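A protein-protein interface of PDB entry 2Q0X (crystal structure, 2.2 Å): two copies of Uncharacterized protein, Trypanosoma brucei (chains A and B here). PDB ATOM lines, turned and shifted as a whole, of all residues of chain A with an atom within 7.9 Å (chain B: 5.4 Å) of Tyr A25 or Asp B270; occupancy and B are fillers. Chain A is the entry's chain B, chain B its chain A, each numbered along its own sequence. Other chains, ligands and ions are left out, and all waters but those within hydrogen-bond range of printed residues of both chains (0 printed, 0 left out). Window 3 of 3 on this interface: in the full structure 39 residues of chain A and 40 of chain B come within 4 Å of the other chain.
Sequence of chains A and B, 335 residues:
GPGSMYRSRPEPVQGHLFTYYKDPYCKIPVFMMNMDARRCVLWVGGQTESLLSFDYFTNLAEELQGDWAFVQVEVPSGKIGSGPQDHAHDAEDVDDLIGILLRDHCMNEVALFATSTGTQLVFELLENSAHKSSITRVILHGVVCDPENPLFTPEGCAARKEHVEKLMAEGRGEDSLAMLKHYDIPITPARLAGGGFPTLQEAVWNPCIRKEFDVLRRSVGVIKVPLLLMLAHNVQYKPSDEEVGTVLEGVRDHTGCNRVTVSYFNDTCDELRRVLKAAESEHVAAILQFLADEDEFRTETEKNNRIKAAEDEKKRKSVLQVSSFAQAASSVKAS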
ATOM      1  N   TYR A  21      -5.886  18.928  17.467  1.00  0.00           N
ATOM      2  CA  TYR A  21      -6.324  20.165  16.844  1.00  0.00           C
ATOM      3  C   TYR A  21      -6.411  19.990  15.338  1.00  0.00           C
ATOM      4  O   TYR A  21      -5.487  19.479  14.711  1.00  0.00           O
ATOM      5  CB  TYR A  21      -5.349  21.299  17.168  1.00  0.00           C
ATOM      6  CG  TYR A  21      -5.729  22.172  18.344  1.00  0.00           C
ATOM      7  CD1 TYR A  21      -6.818  23.039  18.264  1.00  0.00           C
ATOM      8  CD2 TYR A  21      -4.972  22.181  19.513  1.00  0.00           C
ATOM      9  CE1 TYR A  21      -7.165  23.868  19.324  1.00  0.00           C
ATOM     10  CE2 TYR A  21      -5.307  23.018  20.582  1.00  0.00           C
ATOM     11  CZ  TYR A  21      -6.403  23.862  20.481  1.00  0.00           C
ATOM     12  OH  TYR A  21      -6.748  24.698  21.536  1.00  0.00           O
ATOM     13  N   LYS A  22      -7.527  20.427  14.768  1.00  0.00           N
ATOM     14  CA  LYS A  22      -7.732  20.404  13.325  1.00  0.00           C
ATOM     15  C   LYS A  22      -7.167  21.726  12.760  1.00  0.00           C
ATOM     16  O   LYS A  22      -6.007  21.782  12.323  1.00  0.00           O
ATOM     17  CB  LYS A  22      -9.232  20.206  13.023  1.00  0.00           C
ATOM     18  CG  LYS A  22      -9.528  19.661  11.631  1.00  0.00           C
ATOM     19  CD  LYS A  22     -10.591  20.477  10.893  1.00  0.00           C
ATOM     20  CE  LYS A  22     -12.002  19.955  11.159  1.00  0.00           C
ATOM     21  NZ  LYS A  22     -13.069  20.942  10.781  1.00  0.00           N
ATOM     22  N   ASP A  23      -7.999  22.771  12.752  1.00  0.00           N
ATOM     23  CA  ASP A  23      -7.531  24.150  12.833  1.00  0.00           C
ATOM     24  C   ASP A  23      -7.611  24.486  14.332  1.00  0.00           C
ATOM     25  O   ASP A  23      -7.869  23.593  15.134  1.00  0.00           O
ATOM     26  CB  ASP A  23      -8.406  25.061  11.961  1.00  0.00           C
ATOM     27  CG  ASP A  23      -9.794  25.282  12.536  1.00  0.00           C
ATOM     28  OD1 ASP A  23     -10.568  26.058  11.946  1.00  0.00           O
ATOM     29  OD2 ASP A  23     -10.117  24.694  13.575  1.00  0.00           O
ATOM     30  N   PRO A  24      -7.377  25.750  14.729  1.00  0.00           N
ATOM     31  CA  PRO A  24      -7.537  26.081  16.152  1.00  0.00           C
ATOM     32  C   PRO A  24      -8.904  26.710  16.514  1.00  0.00           C
ATOM     33  O   PRO A  24      -8.966  27.691  17.257  1.00  0.00           O
ATOM     34  CB  PRO A  24      -6.390  27.066  16.389  1.00  0.00           C
ATOM     35  CG  PRO A  24      -6.198  27.760  15.026  1.00  0.00           C
ATOM     36  CD  PRO A  24      -6.903  26.919  13.971  1.00  0.00           C
ATOM     37  N   TYR A  25      -9.972  26.165  15.939  1.00  0.00           N
ATOM     38  CA  TYR A  25     -11.347  26.382  16.396  1.00  0.00           C
ATOM     39  C   TYR A  25     -12.111  25.057  16.318  1.00  0.00           C
ATOM     40  O   TYR A  25     -13.344  25.031  16.402  1.00  0.00           O
ATOM     41  CB  TYR A  25     -12.067  27.394  15.499  1.00  0.00           C
ATOM     42  CG  TYR A  25     -11.707  28.838  15.713  1.00  0.00           C
ATOM     43  CD1 TYR A  25     -10.948  29.531  14.771  1.00  0.00           C
ATOM     44  CD2 TYR A  25     -12.158  29.532  16.839  1.00  0.00           C
ATOM     45  CE1 TYR A  25     -10.629  30.864  14.948  1.00  0.00           C
ATOM     46  CE2 TYR A  25     -11.843  30.878  17.025  1.00  0.00           C
ATOM     47  CZ  TYR A  25     -11.076  31.531  16.074  1.00  0.00           C
ATOM     48  OH  TYR A  25     -10.747  32.855  16.236  1.00  0.00           O
ATOM     49  N   CYS A  26     -11.369  23.966  16.147  1.00  0.00           N
ATOM     50  CA  CYS A  26     -11.959  22.656  15.978  1.00  0.00           C
ATOM     51  C   CYS A  26     -11.047  21.608  16.593  1.00  0.00           C
ATOM     52  O   CYS A  26      -9.968  21.318  16.068  1.00  0.00           O
ATOM     53  CB  CYS A  26     -12.180  22.368  14.496  1.00  0.00           C
ATOM     54  SG  CYS A  26     -13.047  20.834  14.195  1.00  0.00           S
ATOM     55  N   LYS A  27     -11.476  21.071  17.729  1.00  0.00           N
ATOM     56  CA  LYS A  27     -10.769  19.993  18.387  1.00  0.00           C
ATOM     57  C   LYS A  27     -11.524  18.712  18.087  1.00  0.00           C
ATOM     58  O   LYS A  27     -12.757  18.715  18.082  1.00  0.00           O
ATOM     59  CB  LYS A  27     -10.738  20.212  19.887  1.00  0.00           C
ATOM     60  CG  LYS A  27      -9.937  21.408  20.335  1.00  0.00           C
ATOM     61  CD  LYS A  27      -9.671  21.333  21.828  1.00  0.00           C
ATOM     62  CE  LYS A  27      -8.929  22.540  22.290  1.00  0.00           C
ATOM     63  NZ  LYS A  27      -8.481  22.346  23.668  1.00  0.00           N
ATOM     64  N   ILE A  28     -10.782  17.635  17.833  1.00  0.00           N
ATOM     65  CA  ILE A  28     -11.353  16.332  17.491  1.00  0.00           C
ATOM     66  C   ILE A  28     -11.130  15.328  18.632  1.00  0.00           C
ATOM     67  O   ILE A  28     -10.000  14.944  18.925  1.00  0.00           O
ATOM     68  CB  ILE A  28     -10.730  15.746  16.198  1.00  0.00           C
ATOM     69  CG1 ILE A  28     -10.993  16.668  15.002  1.00  0.00           C
ATOM     70  CG2 ILE A  28     -11.295  14.363  15.938  1.00  0.00           C
ATOM     71  CD1 ILE A  28     -10.078  16.417  13.787  1.00  0.00           C
ATOM     72  N   ILE A  80     -21.411  20.611  13.527  1.00  0.00           N
ATOM     73  CA  ILE A  80     -21.754  21.919  12.995  1.00  0.00           C
ATOM     74  C   ILE A  80     -20.485  22.754  12.925  1.00  0.00           C
ATOM     75  O   ILE A  80     -19.661  22.698  13.836  1.00  0.00           O
ATOM     76  CB  ILE A  80     -22.832  22.632  13.910  1.00  0.00           C
ATOM     77  CG1 ILE A  80     -24.215  22.584  13.267  1.00  0.00           C
ATOM     78  CG2 ILE A  80     -22.471  24.095  14.199  1.00  0.00           C
ATOM     79  CD1 ILE A  80     -24.753  21.202  13.093  1.00  0.00           C
ATOM     80  N   GLY A  81     -20.315  23.513  11.847  1.00  0.00           N
ATOM     81  CA  GLY A  81     -19.218  24.498  11.761  1.00  0.00           C
ATOM     82  C   GLY A  81     -17.838  23.921  11.461  1.00  0.00           C
ATOM     83  O   GLY A  81     -16.818  24.490  11.844  1.00  0.00           O
ATOM     84  N   SER A  82     -17.803  22.800  10.748  1.00  0.00           N
ATOM     85  CA  SER A  82     -16.544  22.145  10.397  1.00  0.00           C
ATOM     86  C   SER A  82     -15.858  22.739   9.143  1.00  0.00           C
ATOM     87  O   SER A  82     -14.729  22.357   8.821  1.00  0.00           O
ATOM     88  CB  SER A  82     -16.786  20.646  10.203  1.00  0.00           C
ATOM     89  OG  SER A  82     -17.671  20.410   9.120  1.00  0.00           O
ATOM     90  N   THR B  48     -20.223  24.060  18.438  1.00  0.00           N
ATOM     91  CA  THR B  48     -18.930  23.745  17.860  1.00  0.00           C
ATOM     92  C   THR B  48     -17.881  23.413  18.904  1.00  0.00           C
ATOM     93  O   THR B  48     -16.701  23.314  18.582  1.00  0.00           O
ATOM     94  CB  THR B  48     -18.400  24.916  16.990  1.00  0.00           C
ATOM     95  OG1 THR B  48     -18.163  26.064  17.811  1.00  0.00           O
ATOM     96  CG2 THR B  48     -19.406  25.269  15.897  1.00  0.00           C
ATOM     97  N   ASN B 234     -12.607  40.568  24.146  1.00  0.00           N
ATOM     98  CA  ASN B 234     -11.419  40.932  23.364  1.00  0.00           C
ATOM     99  C   ASN B 234     -10.786  42.198  23.937  1.00  0.00           C
ATOM    100  O   ASN B 234     -11.488  43.077  24.436  1.00  0.00           O
ATOM    101  CB  ASN B 234     -11.761  41.146  21.880  1.00  0.00           C
ATOM    102  CG  ASN B 234     -10.539  41.519  21.036  1.00  0.00           C
ATOM    103  OD1 ASN B 234     -10.363  42.672  20.660  1.00  0.00           O
ATOM    104  ND2 ASN B 234      -9.684  40.538  20.750  1.00  0.00           N
ATOM    105  N   THR B 268      -7.828  35.234  26.052  1.00  0.00           N
ATOM    106  CA  THR B 268      -7.593  35.802  24.729  1.00  0.00           C
ATOM    107  C   THR B 268      -8.788  35.424  23.846  1.00  0.00           C
ATOM    108  O   THR B 268      -9.122  34.245  23.703  1.00  0.00           O
ATOM    109  CB  THR B 268      -6.280  35.304  24.141  1.00  0.00           C
ATOM    110  OG1 THR B 268      -5.246  35.505  25.110  1.00  0.00           O
ATOM    111  CG2 THR B 268      -5.951  36.043  22.841  1.00  0.00           C
ATOM    112  N   CYS B 269      -9.449  36.442  23.299  1.00  0.00           N
ATOM    113  CA  CYS B 269     -10.642  36.262  22.486  1.00  0.00           C
ATOM    114  C   CYS B 269     -10.460  36.932  21.140  1.00  0.00           C
ATOM    115  O   CYS B 269      -9.794  37.958  21.048  1.00  0.00           O
ATOM    116  CB  CYS B 269     -11.852  36.867  23.200  1.00  0.00           C
ATOM    117  SG  CYS B 269     -12.052  36.318  24.922  1.00  0.00           S
ATOM    118  N   ASP B 270     -11.041  36.368  20.086  1.00  0.00           N
ATOM    119  CA  ASP B 270     -11.029  37.068  18.804  1.00  0.00           C
ATOM    120  C   ASP B 270     -12.141  38.122  18.812  1.00  0.00           C
ATOM    121  O   ASP B 270     -12.670  38.444  19.877  1.00  0.00           O
ATOM    122  CB  ASP B 270     -11.096  36.088  17.616  1.00  0.00           C
ATOM    123  CG  ASP B 270     -12.410  35.341  17.523  1.00  0.00           C
ATOM    124  OD1 ASP B 270     -13.350  35.679  18.242  1.00  0.00           O
ATOM    125  OD2 ASP B 270     -12.495  34.405  16.706  1.00  0.00           O
ATOM    126  N   GLU B 271     -12.478  38.673  17.650  1.00  0.00           N
ATOM    127  CA  GLU B 271     -13.509  39.692  17.543  1.00  0.00           C
ATOM    128  C   GLU B 271     -14.858  39.078  17.174  1.00  0.00           C
ATOM    129  O   GLU B 271     -15.783  39.792  16.804  1.00  0.00           O
ATOM    130  CB  GLU B 271     -13.103  40.750  16.507  1.00  0.00           C
ATOM    131  N   LEU B 272     -14.982  37.757  17.288  1.00  0.00           N
ATOM    132  CA  LEU B 272     -16.265  37.068  17.059  1.00  0.00           C
ATOM    133  C   LEU B 272     -16.732  36.354  18.330  1.00  0.00           C
ATOM    134  O   LEU B 272     -17.516  35.403  18.279  1.00  0.00           O
ATOM    135  CB  LEU B 272     -16.140  36.108  15.872  1.00  0.00           C
ATOM    136  CG  LEU B 272     -15.879  36.802  14.526  1.00  0.00           C
ATOM    137  CD1 LEU B 272     -15.422  35.784  13.495  1.00  0.00           C
ATOM    138  CD2 LEU B 272     -17.096  37.565  14.011  1.00  0.00           C
ATOM    139  N   ARG B 273     -16.234  36.844  19.465  1.00  0.00           N
ATOM    140  CA  ARG B 273     -16.628  36.392  20.814  1.00  0.00           C
ATOM    141  C   ARG B 273     -16.283  34.926  21.071  1.00  0.00           C
ATOM    142  O   ARG B 273     -16.994  34.235  21.797  1.00  0.00           O
ATOM    143  CB  ARG B 273     -18.107  36.672  21.088  1.00  0.00           C
ATOM    144  CG  ARG B 273     -18.411  38.152  21.215  1.00  0.00           C
ATOM    145  CD  ARG B 273     -19.726  38.409  21.883  1.00  0.00           C
ATOM    146  NE  ARG B 273     -20.838  37.783  21.174  1.00  0.00           N
ATOM    147  CZ  ARG B 273     -21.748  36.994  21.738  1.00  0.00           C
ATOM    148  NH1 ARG B 273     -21.717  36.741  23.031  1.00  0.00           N
ATOM    149  NH2 ARG B 273     -22.709  36.465  21.001  1.00  0.00           N
ATOM    150  N   ARG B 274     -15.168  34.482  20.488  1.00  0.00           N
ATOM    151  CA  ARG B 274     -14.662  33.145  20.684  1.00  0.00           C
ATOM    152  C   ARG B 274     -13.395  33.180  21.539  1.00  0.00           C
ATOM    153  O   ARG B 274     -12.545  34.027  21.359  1.00  0.00           O
ATOM    154  CB  ARG B 274     -14.378  32.517  19.321  1.00  0.00           C
ATOM    155  CG  ARG B 274     -15.614  32.525  18.399  1.00  0.00           C
ATOM    156  CD  ARG B 274     -15.923  31.146  17.853  1.00  0.00           C
ATOM    157  NE  ARG B 274     -15.494  30.998  16.464  1.00  0.00           N
ATOM    158  CZ  ARG B 274     -15.393  29.838  15.818  1.00  0.00           C
ATOM    159  NH1 ARG B 274     -15.649  28.681  16.426  1.00  0.00           N
ATOM    160  NH2 ARG B 274     -15.013  29.838  14.551  1.00  0.00           N
ATOM    161  N   VAL B 275     -13.288  32.266  22.489  1.00  0.00           N
ATOM    162  CA  VAL B 275     -12.094  32.173  23.308  1.00  0.00           C
ATOM    163  C   VAL B 275     -11.019  31.436  22.500  1.00  0.00           C
ATOM    164  O   VAL B 275     -11.224  30.303  22.044  1.00  0.00           O
ATOM    165  CB  VAL B 275     -12.384  31.491  24.674  1.00  0.00           C
ATOM    166  CG1 VAL B 275     -11.106  31.247  25.455  1.00  0.00           C
ATOM    167  CG2 VAL B 275     -13.331  32.345  25.480  1.00  0.00           C
ATOM    168  N   LEU B 276      -9.900  32.118  22.276  1.00  0.00           N
ATOM    169  CA  LEU B 276      -8.744  31.530  21.622  1.00  0.00           C
ATOM    170  C   LEU B 276      -7.847  30.864  22.660  1.00  0.00           C
ATOM    171  O   LEU B 276      -7.234  29.836  22.396  1.00  0.00           O
ATOM    172  CB  LEU B 276      -7.946  32.610  20.874  1.00  0.00           C
ATOM    173  CG  LEU B 276      -8.696  33.387  19.787  1.00  0.00           C
ATOM    174  CD1 LEU B 276      -7.806  34.506  19.209  1.00  0.00           C
ATOM    175  CD2 LEU B 276      -9.185  32.450  18.677  1.00  0.00           C
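OH of Tyr A25 lies close to OD2 of Asp B270 (2.4 Å).
The backbone carbonyl oxygen of Thr B268 lies within hydrogen-bond range of the backbone NH of Leu B276, 2.7 Å away. The backbone NH of Leu B272 lies within hydrogen-bond range of the side-chain carboxylate of Asp B270 (2.8 Å). The side-chain carboxylate (OD1) of Asp B270 sits at hydrogen-bond distance from the backbone NH (N) of Arg B273 (3.3 Å). The backbone NH (N) of Arg B274 sits at hydrogen-bond distance from the side-chain carboxylate (OD1) of Asp B270, 3.1 Å away. OD2 of Asp A23 lies within hydrogen-bond range of N of Tyr A25, 2.8 Å away.
Arg B274 touches Tyr A25. Leu B276 touches Tyr A25 (CD2 to OH, 2.9 Å). O of Ile A80 touches CG2 of Thr B48, at 3.3 Å.
Of chain B, only Asp B270, Arg B274 and Leu B276 come within 4 Å of Tyr A25. Asp B270 touches just one residue of chain A: Tyr A25. Printed residues of chain A within 4 Å of Thr B48: Ile A80 (3.3 Å). Of the printed residues of chain B, Ile A80 touches Thr B48. Of the printed residues of chain A, Leu B276 touches Tyr A25 (2.9 Å). Of the printed residues of chain A, Arg B274 touches Tyr A25 (3.4 Å). Ser A82 touches none of the printed residues of chain B. The nearest residue of chain B that does not touch Tyr A25 is Thr B48 (4.4 Å). The nearest residue of chain A that does not touch Asp B270 is Pro A24 (7.6 Å).
Hydrophobic or aromatic side chains of chain A within 4 Å of the printed part of chain B: Tyr A25 and Ile A80. Of the 11 printed residues of chain B, 4 touch a printed residue of chain A. Among the printed residues, no Asp or Glu carboxylate lies within 4 Å of a Lys or Arg side-chain nitrogen of the other chain.
No position is printed for both chains. Of the 4 pairs that touch across the chains among the printed residues, none has its exchanged pair printed and touching as well.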
